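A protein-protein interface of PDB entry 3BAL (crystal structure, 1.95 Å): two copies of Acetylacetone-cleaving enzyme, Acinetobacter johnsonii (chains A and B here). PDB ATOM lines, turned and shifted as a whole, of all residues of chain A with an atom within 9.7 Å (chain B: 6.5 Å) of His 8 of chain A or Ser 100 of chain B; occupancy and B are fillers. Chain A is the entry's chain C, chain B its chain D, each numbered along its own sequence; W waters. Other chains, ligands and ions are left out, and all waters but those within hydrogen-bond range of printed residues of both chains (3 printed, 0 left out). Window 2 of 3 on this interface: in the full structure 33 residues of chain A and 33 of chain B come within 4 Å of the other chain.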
ATOM      1  N   ASN A   5      24.346 -26.873  20.696  1.00  0.00           N
ATOM      2  CA  ASN A   5      23.425 -27.583  19.810  1.00  0.00           C
ATOM      3  C   ASN A   5      22.209 -28.083  20.587  1.00  0.00           C
ATOM      4  O   ASN A   5      22.340 -28.591  21.695  1.00  0.00           O
ATOM      5  CB  ASN A   5      24.116 -28.774  19.146  1.00  0.00           C
ATOM      6  CG  ASN A   5      25.387 -28.378  18.423  1.00  0.00           C
ATOM      7  OD1 ASN A   5      25.427 -27.363  17.722  1.00  0.00           O
ATOM      8  ND2 ASN A   5      26.430 -29.185  18.576  1.00  0.00           N
ATOM      9  N   LYS A   6      21.029 -27.955  19.993  1.00  0.00           N
ATOM     10  CA  LYS A   6      19.800 -28.392  20.640  1.00  0.00           C
ATOM     11  C   LYS A   6      19.036 -29.437  19.817  1.00  0.00           C
ATOM     12  O   LYS A   6      19.092 -29.450  18.583  1.00  0.00           O
ATOM     13  CB  LYS A   6      18.903 -27.177  20.893  1.00  0.00           C
ATOM     14  CG  LYS A   6      19.524 -26.140  21.832  1.00  0.00           C
ATOM     15  CD  LYS A   6      19.688 -26.696  23.241  1.00  0.00           C
ATOM     16  CE  LYS A   6      20.490 -25.756  24.143  1.00  0.00           C
ATOM     17  NZ  LYS A   6      19.882 -24.394  24.295  1.00  0.00           N
ATOM     18  N   LYS A   7      18.332 -30.319  20.511  1.00  0.00           N
ATOM     19  CA  LYS A   7      17.543 -31.344  19.850  1.00  0.00           C
ATOM     20  C   LYS A   7      16.067 -31.056  20.098  1.00  0.00           C
ATOM     21  O   LYS A   7      15.706 -30.372  21.054  1.00  0.00           O
ATOM     22  CB  LYS A   7      17.895 -32.738  20.385  1.00  0.00           C
ATOM     23  CG  LYS A   7      19.089 -33.413  19.692  1.00  0.00           C
ATOM     24  CD  LYS A   7      20.393 -33.360  20.506  1.00  0.00           C
ATOM     25  CE  LYS A   7      20.979 -31.943  20.606  1.00  0.00           C
ATOM     26  NZ  LYS A   7      22.267 -31.862  21.387  1.00  0.00           N
ATOM     27  N   HIS A   8      15.227 -31.567  19.208  1.00  0.00           N
ATOM     28  CA  HIS A   8      13.779 -31.421  19.292  1.00  0.00           C
ATOM     29  C   HIS A   8      13.321 -31.935  20.672  1.00  0.00           C
ATOM     30  O   HIS A   8      13.767 -32.983  21.140  1.00  0.00           O
ATOM     31  CB  HIS A   8      13.185 -32.217  18.111  1.00  0.00           C
ATOM     32  CG  HIS A   8      11.693 -32.382  18.127  1.00  0.00           C
ATOM     33  ND1 HIS A   8      11.068 -33.472  18.700  1.00  0.00           N
ATOM     34  CD2 HIS A   8      10.710 -31.655  17.539  1.00  0.00           C
ATOM     35  CE1 HIS A   8       9.769 -33.414  18.456  1.00  0.00           C
ATOM     36  NE2 HIS A   8       9.525 -32.322  17.752  1.00  0.00           N
ATOM     37  N   THR A   9      12.469 -31.161  21.339  1.00  0.00           N
ATOM     38  CA  THR A   9      11.955 -31.529  22.653  1.00  0.00           C
ATOM     39  C   THR A   9      10.998 -32.714  22.484  1.00  0.00           C
ATOM     40  O   THR A   9      10.242 -32.776  21.519  1.00  0.00           O
ATOM     41  CB  THR A   9      11.224 -30.324  23.309  1.00  0.00           C
ATOM     42  OG1 THR A   9      12.151 -29.243  23.471  1.00  0.00           O
ATOM     43  CG2 THR A   9      10.652 -30.697  24.673  1.00  0.00           C
ATOM     44  N   ALA A  10      11.044 -33.655  23.418  1.00  0.00           N
ATOM     45  CA  ALA A  10      10.198 -34.848  23.363  1.00  0.00           C
ATOM     46  C   ALA A  10       8.720 -34.540  23.564  1.00  0.00           C
ATOM     47  O   ALA A  10       8.369 -33.710  24.394  1.00  0.00           O
ATOM     48  CB  ALA A  10      10.659 -35.844  24.428  1.00  0.00           C
ATOM     49  N   GLU A  11       7.848 -35.201  22.806  1.00  0.00           N
ATOM     50  CA  GLU A  11       6.416 -34.983  22.998  1.00  0.00           C
ATOM     51  C   GLU A  11       6.004 -35.771  24.246  1.00  0.00           C
ATOM     52  O   GLU A  11       6.701 -36.700  24.652  1.00  0.00           O
ATOM     53  CB  GLU A  11       5.608 -35.461  21.786  1.00  0.00           C
ATOM     54  CG  GLU A  11       5.822 -34.626  20.521  1.00  0.00           C
ATOM     55  CD  GLU A  11       6.933 -35.164  19.636  1.00  0.00           C
ATOM     56  OE1 GLU A  11       7.635 -36.106  20.070  1.00  0.00           O
ATOM     57  OE2 GLU A  11       7.102 -34.649  18.508  1.00  0.00           O
ATOM     58  N   GLU A  12       4.889 -35.404  24.867  1.00  0.00           N
ATOM     59  CA  GLU A  12       4.457 -36.101  26.065  1.00  0.00           C
ATOM     60  C   GLU A  12       2.984 -36.489  26.038  1.00  0.00           C
ATOM     61  O   GLU A  12       2.164 -35.828  25.391  1.00  0.00           O
ATOM     62  CB  GLU A  12       4.709 -35.229  27.298  1.00  0.00           C
ATOM     63  CG  GLU A  12       6.167 -34.905  27.583  1.00  0.00           C
ATOM     64  CD  GLU A  12       6.324 -33.828  28.656  1.00  0.00           C
ATOM     65  OE1 GLU A  12       5.344 -33.565  29.393  1.00  0.00           O
ATOM     66  OE2 GLU A  12       7.427 -33.246  28.776  1.00  0.00           O
ATOM     67  N   SER A  41       7.576 -27.009  32.100  1.00  0.00           N
ATOM     68  CA  SER A  41       8.469 -26.588  31.016  1.00  0.00           C
ATOM     69  C   SER A  41       9.563 -25.775  31.696  1.00  0.00           C
ATOM     70  O   SER A  41       9.442 -24.565  31.850  1.00  0.00           O
ATOM     71  CB  SER A  41       7.739 -25.720  29.994  1.00  0.00           C
ATOM     72  OG  SER A  41       7.151 -26.505  28.968  1.00  0.00           O
ATOM     73  N   GLU A  43      12.412 -24.767  30.689  1.00  0.00           N
ATOM     74  CA  GLU A  43      13.042 -23.783  29.817  1.00  0.00           C
ATOM     75  C   GLU A  43      12.169 -22.535  29.681  1.00  0.00           C
ATOM     76  O   GLU A  43      12.652 -21.409  29.785  1.00  0.00           O
ATOM     77  CB  GLU A  43      13.271 -24.396  28.436  1.00  0.00           C
ATOM     78  CG  GLU A  43      14.174 -23.597  27.513  1.00  0.00           C
ATOM     79  CD  GLU A  43      14.395 -24.294  26.175  1.00  0.00           C
ATOM     80  OE1 GLU A  43      13.466 -24.306  25.339  1.00  0.00           O
ATOM     81  OE2 GLU A  43      15.499 -24.838  25.969  1.00  0.00           O
ATOM     82  N   THR A  44      10.879 -22.761  29.453  1.00  0.00           N
ATOM     83  CA  THR A  44       9.879 -21.702  29.278  1.00  0.00           C
ATOM     84  C   THR A  44       9.433 -21.070  30.609  1.00  0.00           C
ATOM     85  O   THR A  44       9.189 -19.862  30.690  1.00  0.00           O
ATOM     86  CB  THR A  44       8.618 -22.271  28.565  1.00  0.00           C
ATOM     87  OG1 THR A  44       9.007 -22.955  27.365  1.00  0.00           O
ATOM     88  CG2 THR A  44       7.648 -21.155  28.205  1.00  0.00           C
ATOM     89  N   ILE B  63       2.627 -29.035  10.715  1.00  0.00           N
ATOM     90  CA  ILE B  63       3.763 -29.076  11.634  1.00  0.00           C
ATOM     91  C   ILE B  63       3.546 -27.947  12.642  1.00  0.00           C
ATOM     92  O   ILE B  63       3.091 -26.853  12.283  1.00  0.00           O
ATOM     93  CB  ILE B  63       5.112 -28.828  10.898  1.00  0.00           C
ATOM     94  CG1 ILE B  63       5.356 -29.932   9.867  1.00  0.00           C
ATOM     95  CG2 ILE B  63       6.267 -28.803  11.896  1.00  0.00           C
ATOM     96  CD1 ILE B  63       6.579 -29.709   9.014  1.00  0.00           C
ATOM     97  N   HIS B  64       3.855 -28.213  13.906  1.00  0.00           N
ATOM     98  CA  HIS B  64       3.705 -27.201  14.945  1.00  0.00           C
ATOM     99  C   HIS B  64       4.962 -26.359  15.037  1.00  0.00           C
ATOM    100  O   HIS B  64       6.023 -26.862  15.378  1.00  0.00           O
ATOM    101  CB  HIS B  64       3.442 -27.863  16.294  1.00  0.00           C
ATOM    102  CG  HIS B  64       2.045 -28.363  16.448  1.00  0.00           C
ATOM    103  ND1 HIS B  64       1.123 -27.746  17.265  1.00  0.00           N
ATOM    104  CD2 HIS B  64       1.391 -29.378  15.836  1.00  0.00           C
ATOM    105  CE1 HIS B  64      -0.042 -28.358  17.147  1.00  0.00           C
ATOM    106  NE2 HIS B  64       0.094 -29.352  16.284  1.00  0.00           N
ATOM    107  N   ALA B  65       4.838 -25.075  14.729  1.00  0.00           N
ATOM    108  CA  ALA B  65       5.982 -24.184  14.792  1.00  0.00           C
ATOM    109  C   ALA B  65       6.438 -24.005  16.239  1.00  0.00           C
ATOM    110  O   ALA B  65       7.606 -23.723  16.501  1.00  0.00           O
ATOM    111  CB  ALA B  65       5.628 -22.837  14.182  1.00  0.00           C
ATOM    112  N   GLY B  66       5.510 -24.165  17.180  1.00  0.00           N
ATOM    113  CA  GLY B  66       5.842 -24.008  18.589  1.00  0.00           C
ATOM    114  C   GLY B  66       5.104 -25.005  19.460  1.00  0.00           C
ATOM    115  O   GLY B  66       4.290 -25.785  18.957  1.00  0.00           O
ATOM    116  N   PRO B  67       5.343 -24.994  20.778  1.00  0.00           N
ATOM    117  CA  PRO B  67       4.663 -25.938  21.663  1.00  0.00           C
ATOM    118  C   PRO B  67       3.143 -25.767  21.748  1.00  0.00           C
ATOM    119  O   PRO B  67       2.617 -24.648  21.720  1.00  0.00           O
ATOM    120  CB  PRO B  67       5.360 -25.706  23.005  1.00  0.00           C
ATOM    121  CG  PRO B  67       5.677 -24.250  22.960  1.00  0.00           C
ATOM    122  CD  PRO B  67       6.177 -24.054  21.547  1.00  0.00           C
ATOM    123  N   GLY B  68       2.450 -26.900  21.842  1.00  0.00           N
ATOM    124  CA  GLY B  68       1.001 -26.914  21.961  1.00  0.00           C
ATOM    125  C   GLY B  68       0.619 -27.915  23.042  1.00  0.00           C
ATOM    126  O   GLY B  68       1.260 -28.961  23.171  1.00  0.00           O
ATOM    127  N   PHE B  97       1.612 -33.030  25.419  1.00  0.00           N
ATOM    128  CA  PHE B  97       2.491 -31.899  25.104  1.00  0.00           C
ATOM    129  C   PHE B  97       3.089 -32.188  23.727  1.00  0.00           C
ATOM    130  O   PHE B  97       3.856 -33.142  23.560  1.00  0.00           O
ATOM    131  CB  PHE B  97       3.629 -31.758  26.131  1.00  0.00           C
ATOM    132  CG  PHE B  97       4.613 -30.634  25.824  1.00  0.00           C
ATOM    133  CD1 PHE B  97       4.302 -29.305  26.116  1.00  0.00           C
ATOM    134  CD2 PHE B  97       5.860 -30.914  25.258  1.00  0.00           C
ATOM    135  CE1 PHE B  97       5.221 -28.265  25.853  1.00  0.00           C
ATOM    136  CE2 PHE B  97       6.785 -29.884  24.991  1.00  0.00           C
ATOM    137  CZ  PHE B  97       6.462 -28.555  25.291  1.00  0.00           C
ATOM    138  N   GLU B  98       2.719 -31.372  22.745  1.00  0.00           N
ATOM    139  CA  GLU B  98       3.222 -31.523  21.386  1.00  0.00           C
ATOM    140  C   GLU B  98       4.163 -30.352  21.101  1.00  0.00           C
ATOM    141  O   GLU B  98       3.736 -29.229  20.842  1.00  0.00           O
ATOM    142  CB  GLU B  98       2.049 -31.556  20.405  1.00  0.00           C
ATOM    143  CG  GLU B  98       1.120 -32.766  20.607  1.00  0.00           C
ATOM    144  CD  GLU B  98       1.813 -34.089  20.320  1.00  0.00           C
ATOM    145  OE1 GLU B  98       2.552 -34.162  19.318  1.00  0.00           O
ATOM    146  OE2 GLU B  98       1.618 -35.057  21.083  1.00  0.00           O
ATOM    147  N   SER B  99       5.452 -30.651  21.153  1.00  0.00           N
ATOM    148  CA  SER B  99       6.510 -29.673  20.979  1.00  0.00           C
ATOM    149  C   SER B  99       6.731 -29.065  19.595  1.00  0.00           C
ATOM    150  O   SER B  99       6.217 -29.545  18.582  1.00  0.00           O
ATOM    151  CB  SER B  99       7.831 -30.281  21.470  1.00  0.00           C
ATOM    152  OG  SER B  99       8.175 -31.428  20.710  1.00  0.00           O
ATOM    153  N   SER B 100       7.519 -27.990  19.592  1.00  0.00           N
ATOM    154  CA  SER B 100       7.891 -27.268  18.385  1.00  0.00           C
ATOM    155  C   SER B 100       8.570 -28.240  17.425  1.00  0.00           C
ATOM    156  O   SER B 100       9.568 -28.875  17.776  1.00  0.00           O
ATOM    157  CB  SER B 100       8.852 -26.131  18.743  1.00  0.00           C
ATOM    158  OG  SER B 100       9.442 -25.573  17.588  1.00  0.00           O
ATOM    159  N   GLY B 101       8.020 -28.358  16.220  1.00  0.00           N
ATOM    160  CA  GLY B 101       8.576 -29.258  15.222  1.00  0.00           C
ATOM    161  C   GLY B 101       7.767 -30.538  15.091  1.00  0.00           C
ATOM    162  O   GLY B 101       8.047 -31.363  14.221  1.00  0.00           O
ATOM    163  N   ALA B 102       6.758 -30.707  15.944  1.00  0.00           N
ATOM    164  CA  ALA B 102       5.937 -31.914  15.904  1.00  0.00           C
ATOM    165  C   ALA B 102       5.230 -32.061  14.562  1.00  0.00           C
ATOM    166  O   ALA B 102       4.563 -31.138  14.095  1.00  0.00           O
ATOM    167  CB  ALA B 102       4.915 -31.900  17.043  1.00  0.00           C
ATOM    168  N   LEU B 103       5.385 -33.227  13.937  1.00  0.00           N
ATOM    169  CA  LEU B 103       4.752 -33.487  12.645  1.00  0.00           C
ATOM    170  C   LEU B 103       3.475 -34.295  12.817  1.00  0.00           C
ATOM    171  O   LEU B 103       3.511 -35.428  13.293  1.00  0.00           O
ATOM    172  CB  LEU B 103       5.711 -34.238  11.712  1.00  0.00           C
ATOM    173  CG  LEU B 103       5.109 -34.801  10.413  1.00  0.00           C
ATOM    174  CD1 LEU B 103       4.650 -33.671   9.498  1.00  0.00           C
ATOM    175  CD2 LEU B 103       6.143 -35.658   9.713  1.00  0.00           C
HETATM  176  O   HOH W   1      11.115 -28.977  19.984  1.00  0.00           O
HETATM  177  O   HOH W   2       6.897 -35.384  15.473  1.00  0.00           O
HETATM  178  O   HOH W   3       0.563 -36.356  23.252  1.00  0.00           O
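No position is printed for both chains.
Of the 12 pairs that touch across the chains among the printed residues, none has its exchanged pair printed and touching as well.
Water W1 bridges O of Ser 100 of chain B (2.7 Å) and N of Thr 9 of chain A (2.9 Å).
Water W3 bridges the backbone carbonyl oxygen (O) of Glu 12 of chain A (2.7 Å) and the side-chain carboxylate (OE2) of Glu 98 of chain B (2.7 Å).
Water W2 lies within hydrogen-bond range of the backbone NH (N) of Leu 103 of chain B (3.0 Å) and the side-chain carboxylate (OE2) of Glu 11 of chain A (3.1 Å).
A ring nitrogen (NE2) of His 8 of chain A lies within hydrogen-bond range of the side-chain hydroxyl (OG) of Ser 99 of chain B (3.4 Å).
The backbone carbonyl oxygen (O) of Ser 100 of chain B lies close to a ring nitrogen (NE2) of His 8 of chain A, 3.4 Å away.
The backbone carbonyl oxygen (O) of Thr 9 of chain A lies within hydrogen-bond range of the side-chain hydroxyl (OG) of Ser 99 of chain B, 2.6 Å away.
N of Glu 12 of chain A sits at hydrogen-bond distance from O of Phe 97 of chain B (2.8 Å).
Printed residues of chain A within 4 Å of Ser 100 of chain B: His 8.
No residue of chain A comes within 4 Å of Gly 66 of chain B.
Of chain A, only His 8 comes within 4 Å of Gly 101 of chain B.
Printed residues of chain A within 4 Å of Phe 97 of chain B: Thr 9, Ala 10, Glu 11 and Glu 12.
Printed residues of chain A within 4 Å of Glu 98 of chain B: Glu 11.
Glu 43 of chain A touches none of the printed residues of chain B.
The nearest residue of chain B that does not touch His 8 of chain A is Leu 103 of chain B (5.7 Å).
The nearest printed residue of chain B that does not touch Ala 10 of chain A is Ser 99 of chain B (4.3 Å).
His 8 of chain A touches Gly 101 of chain B.
His 8 of chain A touches Ala 102 of chain B.
Thr 9 of chain A touches Phe 97 of chain B (CG2 to CE2, 3.96 Å).
O of Ala 10 of chain A touches CD2 of Phe 97 of chain B, at 3.9 Å.
Phe 97 of chain B touches Glu 11 of chain A.
Glu 11 of chain A touches Glu 98 of chain B (CG to OE1, 3.5 Å).
Glu 11 of chain A touches Ser 99 of chain B.
OE2 of Glu 11 of chain A touches CB of Ala 102 of chain B, 3.8 Å away.
Of the 11 printed residues of chain A, 5 touch a printed residue of chain B.
Printed residues of chain A that touch a printed residue of chain B: His 8, Thr 9, Ala 10, Glu 11 and Glu 12.
Along chain A the printed residues that touch a printed residue of chain B span positions 8 to 12.
Of the 13 printed residues of chain B, 6 touch a printed residue of chain A.
Among the printed residues, no Asp or Glu carboxylate lies within 4 Å of a Lys or Arg side-chain nitrogen of the other chain.
A ring nitrogen (NE2) of His 8 of chain A lies close to the side-chain carboxylate (OE2) of Glu 11 of chain A (3.4 Å).
The backbone carbonyl oxygen of His 64 of chain B lies within hydrogen-bond range of the backbone NH of Gly 101 of chain B (2.6 Å).
O of Ala 102 of chain B is in hydrogen-bond range of N of His 64 of chain B.
O of Ala 65 of chain B is in hydrogen-bond range of OG of Ser 100 of chain B.
The backbone carbonyl oxygen (O) of Glu 98 of chain B sits at hydrogen-bond distance from the backbone NH (N) of Gly 68 of chain B.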
